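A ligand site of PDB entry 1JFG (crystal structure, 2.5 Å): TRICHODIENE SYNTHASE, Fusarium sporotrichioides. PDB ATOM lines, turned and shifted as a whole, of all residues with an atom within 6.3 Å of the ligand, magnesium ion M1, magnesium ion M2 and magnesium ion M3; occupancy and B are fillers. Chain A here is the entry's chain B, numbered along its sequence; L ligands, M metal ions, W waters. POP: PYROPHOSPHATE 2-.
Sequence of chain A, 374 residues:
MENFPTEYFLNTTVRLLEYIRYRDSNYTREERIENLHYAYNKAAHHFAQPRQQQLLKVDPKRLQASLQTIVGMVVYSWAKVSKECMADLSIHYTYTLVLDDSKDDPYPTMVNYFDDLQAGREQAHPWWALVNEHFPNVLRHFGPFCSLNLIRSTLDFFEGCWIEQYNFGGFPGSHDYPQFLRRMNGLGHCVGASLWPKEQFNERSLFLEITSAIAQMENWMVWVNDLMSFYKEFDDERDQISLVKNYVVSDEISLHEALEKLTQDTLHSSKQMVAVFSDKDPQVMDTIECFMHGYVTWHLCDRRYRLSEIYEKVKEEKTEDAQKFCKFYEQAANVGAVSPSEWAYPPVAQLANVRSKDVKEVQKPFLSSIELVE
The side-chain hydroxyl of Ser 229 sits at hydrogen-bond distance from the backbone carbonyl oxygen of Asn 225, 2.6 Å away.
The side-chain hydroxyl (OG) of Ser 229 sits close to the side-chain carboxylate (OE2) of Glu 233, at 3.2 Å.
The side-chain amide nitrogen (ND2) of Asn 185 lies within hydrogen-bond range of the side-chain carboxylate (OE2) of Glu 164 (3.0 Å).
The side-chain amide nitrogen of Asn 225 sits at hydrogen-bond distance from the side-chain hydroxyl of Tyr 305, 3.4 Å away.
NZ of Lys 232 is in salt-bridge range of OD2 of Asp 239 (3.1 Å).
OE1 of Glu 164 is in salt-bridge range of NH2 of Arg 238, at 2.4 Å.
NH2 of Arg 182 is in hydrogen-bond range of O of Val 222, 3.0 Å away.
The side-chain amide oxygen of Asn 225 sits close to the guanidinium group of Arg 182, at 3.3 Å.
Magnesium ion M2 is bound by water W5 (1.9 Å), water W4 (2.1 Å), O5 of the ligand (2.2 Å), O2 of the ligand (2.2 Å), water W1 (2.3 Å) and OD2 of Asp 100 (2.3 Å).
Magnesium ion M2 has six donor atoms within binding distance.
Glu 164 touches magnesium ion M3 (OE1 to MG, 3.4 Å).
CB of Asn 185 touches magnesium ion M3, 3.8 Å away.
Within 4 Å of magnesium ion M3: Asp 100, Glu 164 and Asn 185.
Along chain A the residues within 4 Å of magnesium ion M3 span positions 100 to 185.
An oxygen (O3) of the ligand lies within salt-bridge range of the guanidinium group (NH1) of Arg 182 (2.9 Å).
OH of Tyr 305 lies within hydrogen-bond range of O6 of the ligand, at 2.7 Å.
OG of Ser 229 sits close to O4 of the ligand (3.3 Å).
The guanidinium group of Arg 304 lies within salt-bridge range of an oxygen (O6) of the ligand.
The side-chain amino group of Lys 232 lies close to an oxygen (O5) of the ligand (3.1 Å).
Water W2 lies within hydrogen-bond range of OD1 of Asp 226, OE1 of Glu 233 and OG of Ser 229.
Water W5 lies within hydrogen-bond range of OD1 of Asp 239 (2.6 Å), OD1 of Asp 101 (2.6 Å), NH2 of Arg 304 (3.3 Å) and NZ of Lys 232 (3.4 Å).
Water W3 bridges an oxygen (O3) of the ligand (2.7 Å) and the backbone carbonyl oxygen of Asn 185 (2.7 Å).
Water W2 is bound to magnesium ion M1 (1.8 Å).
OE2 of Glu 233 binds magnesium ion M1, at 2.0 Å.
An oxygen (O4) of the ligand binds magnesium ion M1 (2.0 Å).
Magnesium ion M1 is bound by an oxygen (O1) of the ligand (2.2 Å).
OD1 of Asn 225 is bound to magnesium ion M1 (2.5 Å).
Slightly farther from magnesium ion M1 lies the side-chain hydroxyl (OG) of Ser 229 (2.8 Å).
Water W3 is bound to magnesium ion M3 (1.9 Å).
OD1 of Asp 100 is bound to magnesium ion M3 (2.3 Å).
An oxygen (O2) of the ligand is bound to magnesium ion M3 (2.3 Å).
Magnesium ion M3 has three donor atoms within binding distance.
Slightly farther from magnesium ion M3 lies water W1 (2.6 Å).
OD1 of Asp 239 touches magnesium ion M2, at 3.8 Å.
NH2 of Arg 304 touches magnesium ion M2, 3.7 Å away.
Within 4 Å of the ligand: Asp 100, Arg 182, Asn 225, Ser 229, Lys 232, Glu 233, Arg 304 and Tyr 305.
The nearest printed residue that does not touch the ligand is Asn 185 (4.1 Å).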
ATOM      1  N   LEU A  97     -32.929  22.351   5.346  1.00  0.00           N
ATOM      2  CA  LEU A  97     -32.551  22.018   6.715  1.00  0.00           C
ATOM      3  C   LEU A  97     -31.872  20.649   6.814  1.00  0.00           C
ATOM      4  O   LEU A  97     -30.931  20.474   7.597  1.00  0.00           O
ATOM      5  CB  LEU A  97     -33.772  22.045   7.607  1.00  0.00           C
ATOM      6  CG  LEU A  97     -33.467  21.859   9.098  1.00  0.00           C
ATOM      7  CD1 LEU A  97     -32.435  22.893   9.532  1.00  0.00           C
ATOM      8  CD2 LEU A  97     -34.732  22.009   9.913  1.00  0.00           C
ATOM      9  N   ASP A 100     -28.596  21.419   5.934  1.00  0.00           N
ATOM     10  CA  ASP A 100     -28.068  22.375   6.911  1.00  0.00           C
ATOM     11  C   ASP A 100     -27.314  21.732   8.080  1.00  0.00           C
ATOM     12  O   ASP A 100     -26.345  22.303   8.595  1.00  0.00           O
ATOM     13  CB  ASP A 100     -29.210  23.251   7.460  1.00  0.00           C
ATOM     14  CG  ASP A 100     -28.737  24.324   8.442  1.00  0.00           C
ATOM     15  OD1 ASP A 100     -28.055  25.275   8.014  1.00  0.00           O
ATOM     16  OD2 ASP A 100     -29.058  24.220   9.651  1.00  0.00           O
ATOM     17  N   ASP A 101     -27.757  20.552   8.507  1.00  0.00           N
ATOM     18  CA  ASP A 101     -27.111  19.845   9.613  1.00  0.00           C
ATOM     19  C   ASP A 101     -26.338  18.646   9.108  1.00  0.00           C
ATOM     20  O   ASP A 101     -25.757  17.895   9.890  1.00  0.00           O
ATOM     21  CB  ASP A 101     -28.133  19.343  10.635  1.00  0.00           C
ATOM     22  CG  ASP A 101     -28.915  20.454  11.299  1.00  0.00           C
ATOM     23  OD1 ASP A 101     -28.312  21.454  11.763  1.00  0.00           O
ATOM     24  OD2 ASP A 101     -30.151  20.323  11.382  1.00  0.00           O
ATOM     25  N   PHE A 157     -27.000  28.780  -0.719  1.00  0.00           N
ATOM     26  CA  PHE A 157     -27.116  27.894   0.437  1.00  0.00           C
ATOM     27  C   PHE A 157     -26.286  26.635   0.269  1.00  0.00           C
ATOM     28  O   PHE A 157     -25.602  26.203   1.193  1.00  0.00           O
ATOM     29  CB  PHE A 157     -28.590  27.520   0.659  1.00  0.00           C
ATOM     30  CG  PHE A 157     -28.807  26.610   1.843  1.00  0.00           C
ATOM     31  CD1 PHE A 157     -28.638  27.092   3.137  1.00  0.00           C
ATOM     32  CD2 PHE A 157     -29.159  25.275   1.646  1.00  0.00           C
ATOM     33  CE1 PHE A 157     -28.817  26.261   4.229  1.00  0.00           C
ATOM     34  CE2 PHE A 157     -29.342  24.423   2.745  1.00  0.00           C
ATOM     35  CZ  PHE A 157     -29.174  24.921   4.045  1.00  0.00           C
ATOM     36  N   CYS A 161     -23.195  25.362   2.702  1.00  0.00           N
ATOM     37  CA  CYS A 161     -23.064  24.075   3.370  1.00  0.00           C
ATOM     38  C   CYS A 161     -21.726  23.425   3.001  1.00  0.00           C
ATOM     39  O   CYS A 161     -21.106  22.760   3.842  1.00  0.00           O
ATOM     40  CB  CYS A 161     -24.205  23.145   2.953  1.00  0.00           C
ATOM     41  SG  CYS A 161     -25.809  23.698   3.602  1.00  0.00           S
ATOM     42  N   GLU A 164     -18.997  25.184   4.939  1.00  0.00           N
ATOM     43  CA  GLU A 164     -19.075  24.807   6.345  1.00  0.00           C
ATOM     44  C   GLU A 164     -18.516  23.425   6.649  1.00  0.00           C
ATOM     45  O   GLU A 164     -18.188  23.140   7.802  1.00  0.00           O
ATOM     46  CB  GLU A 164     -20.519  24.908   6.843  1.00  0.00           C
ATOM     47  CG  GLU A 164     -21.060  26.324   6.740  1.00  0.00           C
ATOM     48  CD  GLU A 164     -22.450  26.485   7.324  1.00  0.00           C
ATOM     49  OE1 GLU A 164     -23.360  25.682   6.990  1.00  0.00           O
ATOM     50  OE2 GLU A 164     -22.642  27.429   8.124  1.00  0.00           O
ATOM     51  N   ARG A 182     -22.373  34.002   6.369  1.00  0.00           N
ATOM     52  CA  ARG A 182     -23.732  34.075   6.892  1.00  0.00           C
ATOM     53  C   ARG A 182     -24.767  34.327   5.788  1.00  0.00           C
ATOM     54  O   ARG A 182     -25.884  33.810   5.856  1.00  0.00           O
ATOM     55  CB  ARG A 182     -23.818  35.138   7.987  1.00  0.00           C
ATOM     56  CG  ARG A 182     -25.164  35.163   8.719  1.00  0.00           C
ATOM     57  CD  ARG A 182     -25.669  33.755   9.016  1.00  0.00           C
ATOM     58  NE  ARG A 182     -26.833  33.763   9.886  1.00  0.00           N
ATOM     59  CZ  ARG A 182     -27.635  32.725  10.048  1.00  0.00           C
ATOM     60  NH1 ARG A 182     -27.410  31.596   9.381  1.00  0.00           N
ATOM     61  NH2 ARG A 182     -28.677  32.808  10.869  1.00  0.00           N
ATOM     62  N   ASN A 185     -25.254  30.945   3.609  1.00  0.00           N
ATOM     63  CA  ASN A 185     -26.134  29.944   4.209  1.00  0.00           C
ATOM     64  C   ASN A 185     -27.440  30.463   4.803  1.00  0.00           C
ATOM     65  O   ASN A 185     -28.255  29.683   5.296  1.00  0.00           O
ATOM     66  CB  ASN A 185     -25.382  29.199   5.321  1.00  0.00           C
ATOM     67  CG  ASN A 185     -24.994  30.111   6.483  1.00  0.00           C
ATOM     68  OD1 ASN A 185     -25.796  30.925   6.943  1.00  0.00           O
ATOM     69  ND2 ASN A 185     -23.768  29.970   6.961  1.00  0.00           N
ATOM     70  N   GLY A 186     -27.650  31.775   4.747  1.00  0.00           N
ATOM     71  CA  GLY A 186     -28.829  32.376   5.338  1.00  0.00           C
ATOM     72  C   GLY A 186     -30.176  32.188   4.673  1.00  0.00           C
ATOM     73  O   GLY A 186     -31.183  32.262   5.350  1.00  0.00           O
ATOM     74  N   VAL A 222     -31.682  36.722   9.365  1.00  0.00           N
ATOM     75  CA  VAL A 222     -30.547  35.906   9.792  1.00  0.00           C
ATOM     76  C   VAL A 222     -29.990  36.306  11.150  1.00  0.00           C
ATOM     77  O   VAL A 222     -29.604  35.448  11.955  1.00  0.00           O
ATOM     78  CB  VAL A 222     -29.382  35.943   8.777  1.00  0.00           C
ATOM     79  CG1 VAL A 222     -29.826  35.342   7.473  1.00  0.00           C
ATOM     80  CG2 VAL A 222     -28.902  37.361   8.587  1.00  0.00           C
ATOM     81  N   ASN A 225     -32.242  35.115  13.998  1.00  0.00           N
ATOM     82  CA  ASN A 225     -32.019  33.694  14.263  1.00  0.00           C
ATOM     83  C   ASN A 225     -30.676  33.475  14.951  1.00  0.00           C
ATOM     84  O   ASN A 225     -30.533  32.571  15.771  1.00  0.00           O
ATOM     85  CB  ASN A 225     -32.066  32.880  12.977  1.00  0.00           C
ATOM     86  CG  ASN A 225     -31.715  31.415  13.200  1.00  0.00           C
ATOM     87  OD1 ASN A 225     -30.606  30.970  12.899  1.00  0.00           O
ATOM     88  ND2 ASN A 225     -32.648  30.667  13.751  1.00  0.00           N
ATOM     89  N   ASP A 226     -29.675  34.275  14.612  1.00  0.00           N
ATOM     90  CA  ASP A 226     -28.374  34.142  15.257  1.00  0.00           C
ATOM     91  C   ASP A 226     -28.468  34.465  16.745  1.00  0.00           C
ATOM     92  O   ASP A 226     -27.808  33.821  17.569  1.00  0.00           O
ATOM     93  CB  ASP A 226     -27.350  35.068  14.601  1.00  0.00           C
ATOM     94  CG  ASP A 226     -26.736  34.468  13.357  1.00  0.00           C
ATOM     95  OD1 ASP A 226     -26.391  33.273  13.386  1.00  0.00           O
ATOM     96  OD2 ASP A 226     -26.571  35.187  12.355  1.00  0.00           O
ATOM     97  N   SER A 229     -31.011  31.757  18.463  1.00  0.00           N
ATOM     98  CA  SER A 229     -30.427  30.407  18.438  1.00  0.00           C
ATOM     99  C   SER A 229     -28.967  30.315  18.874  1.00  0.00           C
ATOM    100  O   SER A 229     -28.288  29.332  18.574  1.00  0.00           O
ATOM    101  CB  SER A 229     -30.564  29.780  17.037  1.00  0.00           C
ATOM    102  OG  SER A 229     -29.558  30.236  16.145  1.00  0.00           O
ATOM    103  N   PHE A 230     -28.484  31.335  19.570  1.00  0.00           N
ATOM    104  CA  PHE A 230     -27.106  31.305  20.043  1.00  0.00           C
ATOM    105  C   PHE A 230     -26.940  30.161  21.043  1.00  0.00           C
ATOM    106  O   PHE A 230     -25.870  29.573  21.161  1.00  0.00           O
ATOM    107  CB  PHE A 230     -26.744  32.633  20.714  1.00  0.00           C
ATOM    108  CG  PHE A 230     -25.381  32.634  21.339  1.00  0.00           C
ATOM    109  CD1 PHE A 230     -24.261  32.297  20.595  1.00  0.00           C
ATOM    110  CD2 PHE A 230     -25.221  32.975  22.683  1.00  0.00           C
ATOM    111  CE1 PHE A 230     -22.989  32.296  21.172  1.00  0.00           C
ATOM    112  CE2 PHE A 230     -23.955  32.978  23.266  1.00  0.00           C
ATOM    113  CZ  PHE A 230     -22.836  32.633  22.510  1.00  0.00           C
ATOM    114  N   LYS A 232     -28.698  26.928  21.317  1.00  0.00           N
ATOM    115  CA  LYS A 232     -28.598  25.576  20.788  1.00  0.00           C
ATOM    116  C   LYS A 232     -27.351  25.293  19.948  1.00  0.00           C
ATOM    117  O   LYS A 232     -26.960  24.136  19.791  1.00  0.00           O
ATOM    118  CB  LYS A 232     -29.863  25.212  19.994  1.00  0.00           C
ATOM    119  CG  LYS A 232     -29.956  25.805  18.603  1.00  0.00           C
ATOM    120  CD  LYS A 232     -29.353  24.888  17.544  1.00  0.00           C
ATOM    121  CE  LYS A 232     -29.489  25.485  16.152  1.00  0.00           C
ATOM    122  NZ  LYS A 232     -28.984  24.602  15.080  1.00  0.00           N
ATOM    123  N   GLU A 233     -26.726  26.333  19.415  1.00  0.00           N
ATOM    124  CA  GLU A 233     -25.537  26.138  18.592  1.00  0.00           C
ATOM    125  C   GLU A 233     -24.246  26.276  19.409  1.00  0.00           C
ATOM    126  O   GLU A 233     -23.193  25.788  19.010  1.00  0.00           O
ATOM    127  CB  GLU A 233     -25.485  27.170  17.448  1.00  0.00           C
ATOM    128  CG  GLU A 233     -26.757  27.318  16.625  1.00  0.00           C
ATOM    129  CD  GLU A 233     -26.631  28.342  15.502  1.00  0.00           C
ATOM    130  OE1 GLU A 233     -25.670  29.150  15.516  1.00  0.00           O
ATOM    131  OE2 GLU A 233     -27.490  28.357  14.596  1.00  0.00           O
ATOM    132  N   ARG A 238     -21.348  20.650  14.880  1.00  0.00           N
ATOM    133  CA  ARG A 238     -21.690  21.061  13.525  1.00  0.00           C
ATOM    134  C   ARG A 238     -21.975  22.558  13.416  1.00  0.00           C
ATOM    135  O   ARG A 238     -21.898  23.141  12.332  1.00  0.00           O
ATOM    136  CB  ARG A 238     -22.893  20.231  13.037  1.00  0.00           C
ATOM    137  CG  ARG A 238     -23.621  20.749  11.792  1.00  0.00           C
ATOM    138  CD  ARG A 238     -22.760  20.783  10.537  1.00  0.00           C
ATOM    139  NE  ARG A 238     -22.781  22.111   9.931  1.00  0.00           N
ATOM    140  CZ  ARG A 238     -23.096  22.360   8.673  1.00  0.00           C
ATOM    141  NH1 ARG A 238     -23.416  21.370   7.854  1.00  0.00           N
ATOM    142  NH2 ARG A 238     -23.098  23.604   8.223  1.00  0.00           N
ATOM    143  N   ASP A 239     -22.314  23.191  14.531  1.00  0.00           N
ATOM    144  CA  ASP A 239     -22.630  24.623  14.532  1.00  0.00           C
ATOM    145  C   ASP A 239     -21.578  25.507  15.203  1.00  0.00           C
ATOM    146  O   ASP A 239     -21.842  26.678  15.485  1.00  0.00           O
ATOM    147  CB  ASP A 239     -23.981  24.903  15.203  1.00  0.00           C
ATOM    148  CG  ASP A 239     -25.125  24.125  14.581  1.00  0.00           C
ATOM    149  OD1 ASP A 239     -25.124  23.919  13.352  1.00  0.00           O
ATOM    150  OD2 ASP A 239     -26.053  23.727  15.325  1.00  0.00           O
ATOM    151  N   TRP A 298     -42.057  31.541  16.727  1.00  0.00           N
ATOM    152  CA  TRP A 298     -41.515  30.244  16.370  1.00  0.00           C
ATOM    153  C   TRP A 298     -40.261  29.901  17.168  1.00  0.00           C
ATOM    154  O   TRP A 298     -40.109  28.796  17.687  1.00  0.00           O
ATOM    155  CB  TRP A 298     -41.209  30.206  14.880  1.00  0.00           C
ATOM    156  CG  TRP A 298     -40.594  28.925  14.422  1.00  0.00           C
ATOM    157  CD1 TRP A 298     -41.138  27.668  14.507  1.00  0.00           C
ATOM    158  CD2 TRP A 298     -39.315  28.765  13.797  1.00  0.00           C
ATOM    159  NE1 TRP A 298     -40.275  26.738  13.971  1.00  0.00           N
ATOM    160  CE2 TRP A 298     -39.155  27.386  13.529  1.00  0.00           C
ATOM    161  CE3 TRP A 298     -38.304  29.652  13.439  1.00  0.00           C
ATOM    162  CZ2 TRP A 298     -38.004  26.880  12.905  1.00  0.00           C
ATOM    163  CZ3 TRP A 298     -37.159  29.149  12.822  1.00  0.00           C
ATOM    164  CH2 TRP A 298     -37.020  27.772  12.562  1.00  0.00           C
ATOM    165  N   HIS A 299     -39.351  30.859  17.267  1.00  0.00           N
ATOM    166  CA  HIS A 299     -38.115  30.638  18.013  1.00  0.00           C
ATOM    167  C   HIS A 299     -38.373  30.335  19.485  1.00  0.00           C
ATOM    168  O   HIS A 299     -37.765  29.435  20.051  1.00  0.00           O
ATOM    169  CB  HIS A 299     -37.199  31.851  17.894  1.00  0.00           C
ATOM    170  CG  HIS A 299     -36.476  31.928  16.595  1.00  0.00           C
ATOM    171  ND1 HIS A 299     -35.224  31.396  16.414  1.00  0.00           N
ATOM    172  CD2 HIS A 299     -36.823  32.499  15.412  1.00  0.00           C
ATOM    173  CE1 HIS A 299     -34.826  31.627  15.172  1.00  0.00           C
ATOM    174  NE2 HIS A 299     -35.773  32.286  14.546  1.00  0.00           N
ATOM    175  N   ARG A 304     -36.095  22.563  18.254  1.00  0.00           N
ATOM    176  CA  ARG A 304     -34.756  22.746  17.730  1.00  0.00           C
ATOM    177  C   ARG A 304     -33.909  23.801  18.450  1.00  0.00           C
ATOM    178  O   ARG A 304     -32.691  23.643  18.576  1.00  0.00           O
ATOM    179  CB  ARG A 304     -34.832  23.079  16.247  1.00  0.00           C
ATOM    180  CG  ARG A 304     -33.500  23.138  15.533  1.00  0.00           C
ATOM    181  CD  ARG A 304     -33.699  23.732  14.154  1.00  0.00           C
ATOM    182  NE  ARG A 304     -32.444  23.980  13.446  1.00  0.00           N
ATOM    183  CZ  ARG A 304     -31.739  23.037  12.829  1.00  0.00           C
ATOM    184  NH1 ARG A 304     -32.150  21.778  12.824  1.00  0.00           N
ATOM    185  NH2 ARG A 304     -30.615  23.370  12.187  1.00  0.00           N
ATOM    186  N   TYR A 305     -34.546  24.862  18.954  1.00  0.00           N
ATOM    187  CA  TYR A 305     -33.798  25.927  19.628  1.00  0.00           C
ATOM    188  C   TYR A 305     -33.679  25.825  21.143  1.00  0.00           C
ATOM    189  O   TYR A 305     -33.102  26.716  21.791  1.00  0.00           O
ATOM    190  CB  TYR A 305     -34.388  27.285  19.211  1.00  0.00           C
ATOM    191  CG  TYR A 305     -34.313  27.465  17.720  1.00  0.00           C
ATOM    192  CD1 TYR A 305     -33.076  27.453  17.052  1.00  0.00           C
ATOM    193  CD2 TYR A 305     -35.471  27.535  16.950  1.00  0.00           C
ATOM    194  CE1 TYR A 305     -33.002  27.485  15.667  1.00  0.00           C
ATOM    195  CE2 TYR A 305     -35.407  27.579  15.549  1.00  0.00           C
ATOM    196  CZ  TYR A 305     -34.170  27.546  14.922  1.00  0.00           C
ATOM    197  OH  TYR A 305     -34.092  27.545  13.543  1.00  0.00           O
HETATM  198  P1  POP L   1     -28.571  28.435  10.472  1.00  0.00           P
HETATM  199  O1  POP L   1     -27.921  29.288  11.554  1.00  0.00           O
HETATM  200  O2  POP L   1     -27.619  27.370  10.039  1.00  0.00           O
HETATM  201  O3  POP L   1     -29.046  29.201   9.301  1.00  0.00           O
HETATM  202  O   POP L   1     -30.016  28.039  11.075  1.00  0.00           O
HETATM  203  P2  POP L   1     -30.276  27.199  12.454  1.00  0.00           P
HETATM  204  O4  POP L   1     -29.791  28.002  13.682  1.00  0.00           O
HETATM  205  O5  POP L   1     -29.528  25.891  12.272  1.00  0.00           O
HETATM  206  O6  POP L   1     -31.710  27.104  12.465  1.00  0.00           O
HETATM  207 MG    MG M   1     -28.645  29.651  13.591  1.00  0.00          MG
HETATM  208 MG    MG M   2     -27.719  25.417  11.089  1.00  0.00          MG
HETATM  209 MG    MG M   3     -26.378  26.840   8.122  1.00  0.00          MG
HETATM  210  O   HOH W   1     -26.184  24.652   9.602  1.00  0.00           O
HETATM  211  O   HOH W   2     -27.456  31.021  13.829  1.00  0.00           O
HETATM  212  O   HOH W   3     -27.725  27.953   7.349  1.00  0.00           O
HETATM  213  O   HOH W   4     -26.689  26.487  12.516  1.00  0.00           O
HETATM  214  O   HOH W   5     -27.385  23.901  12.151  1.00  0.00           O
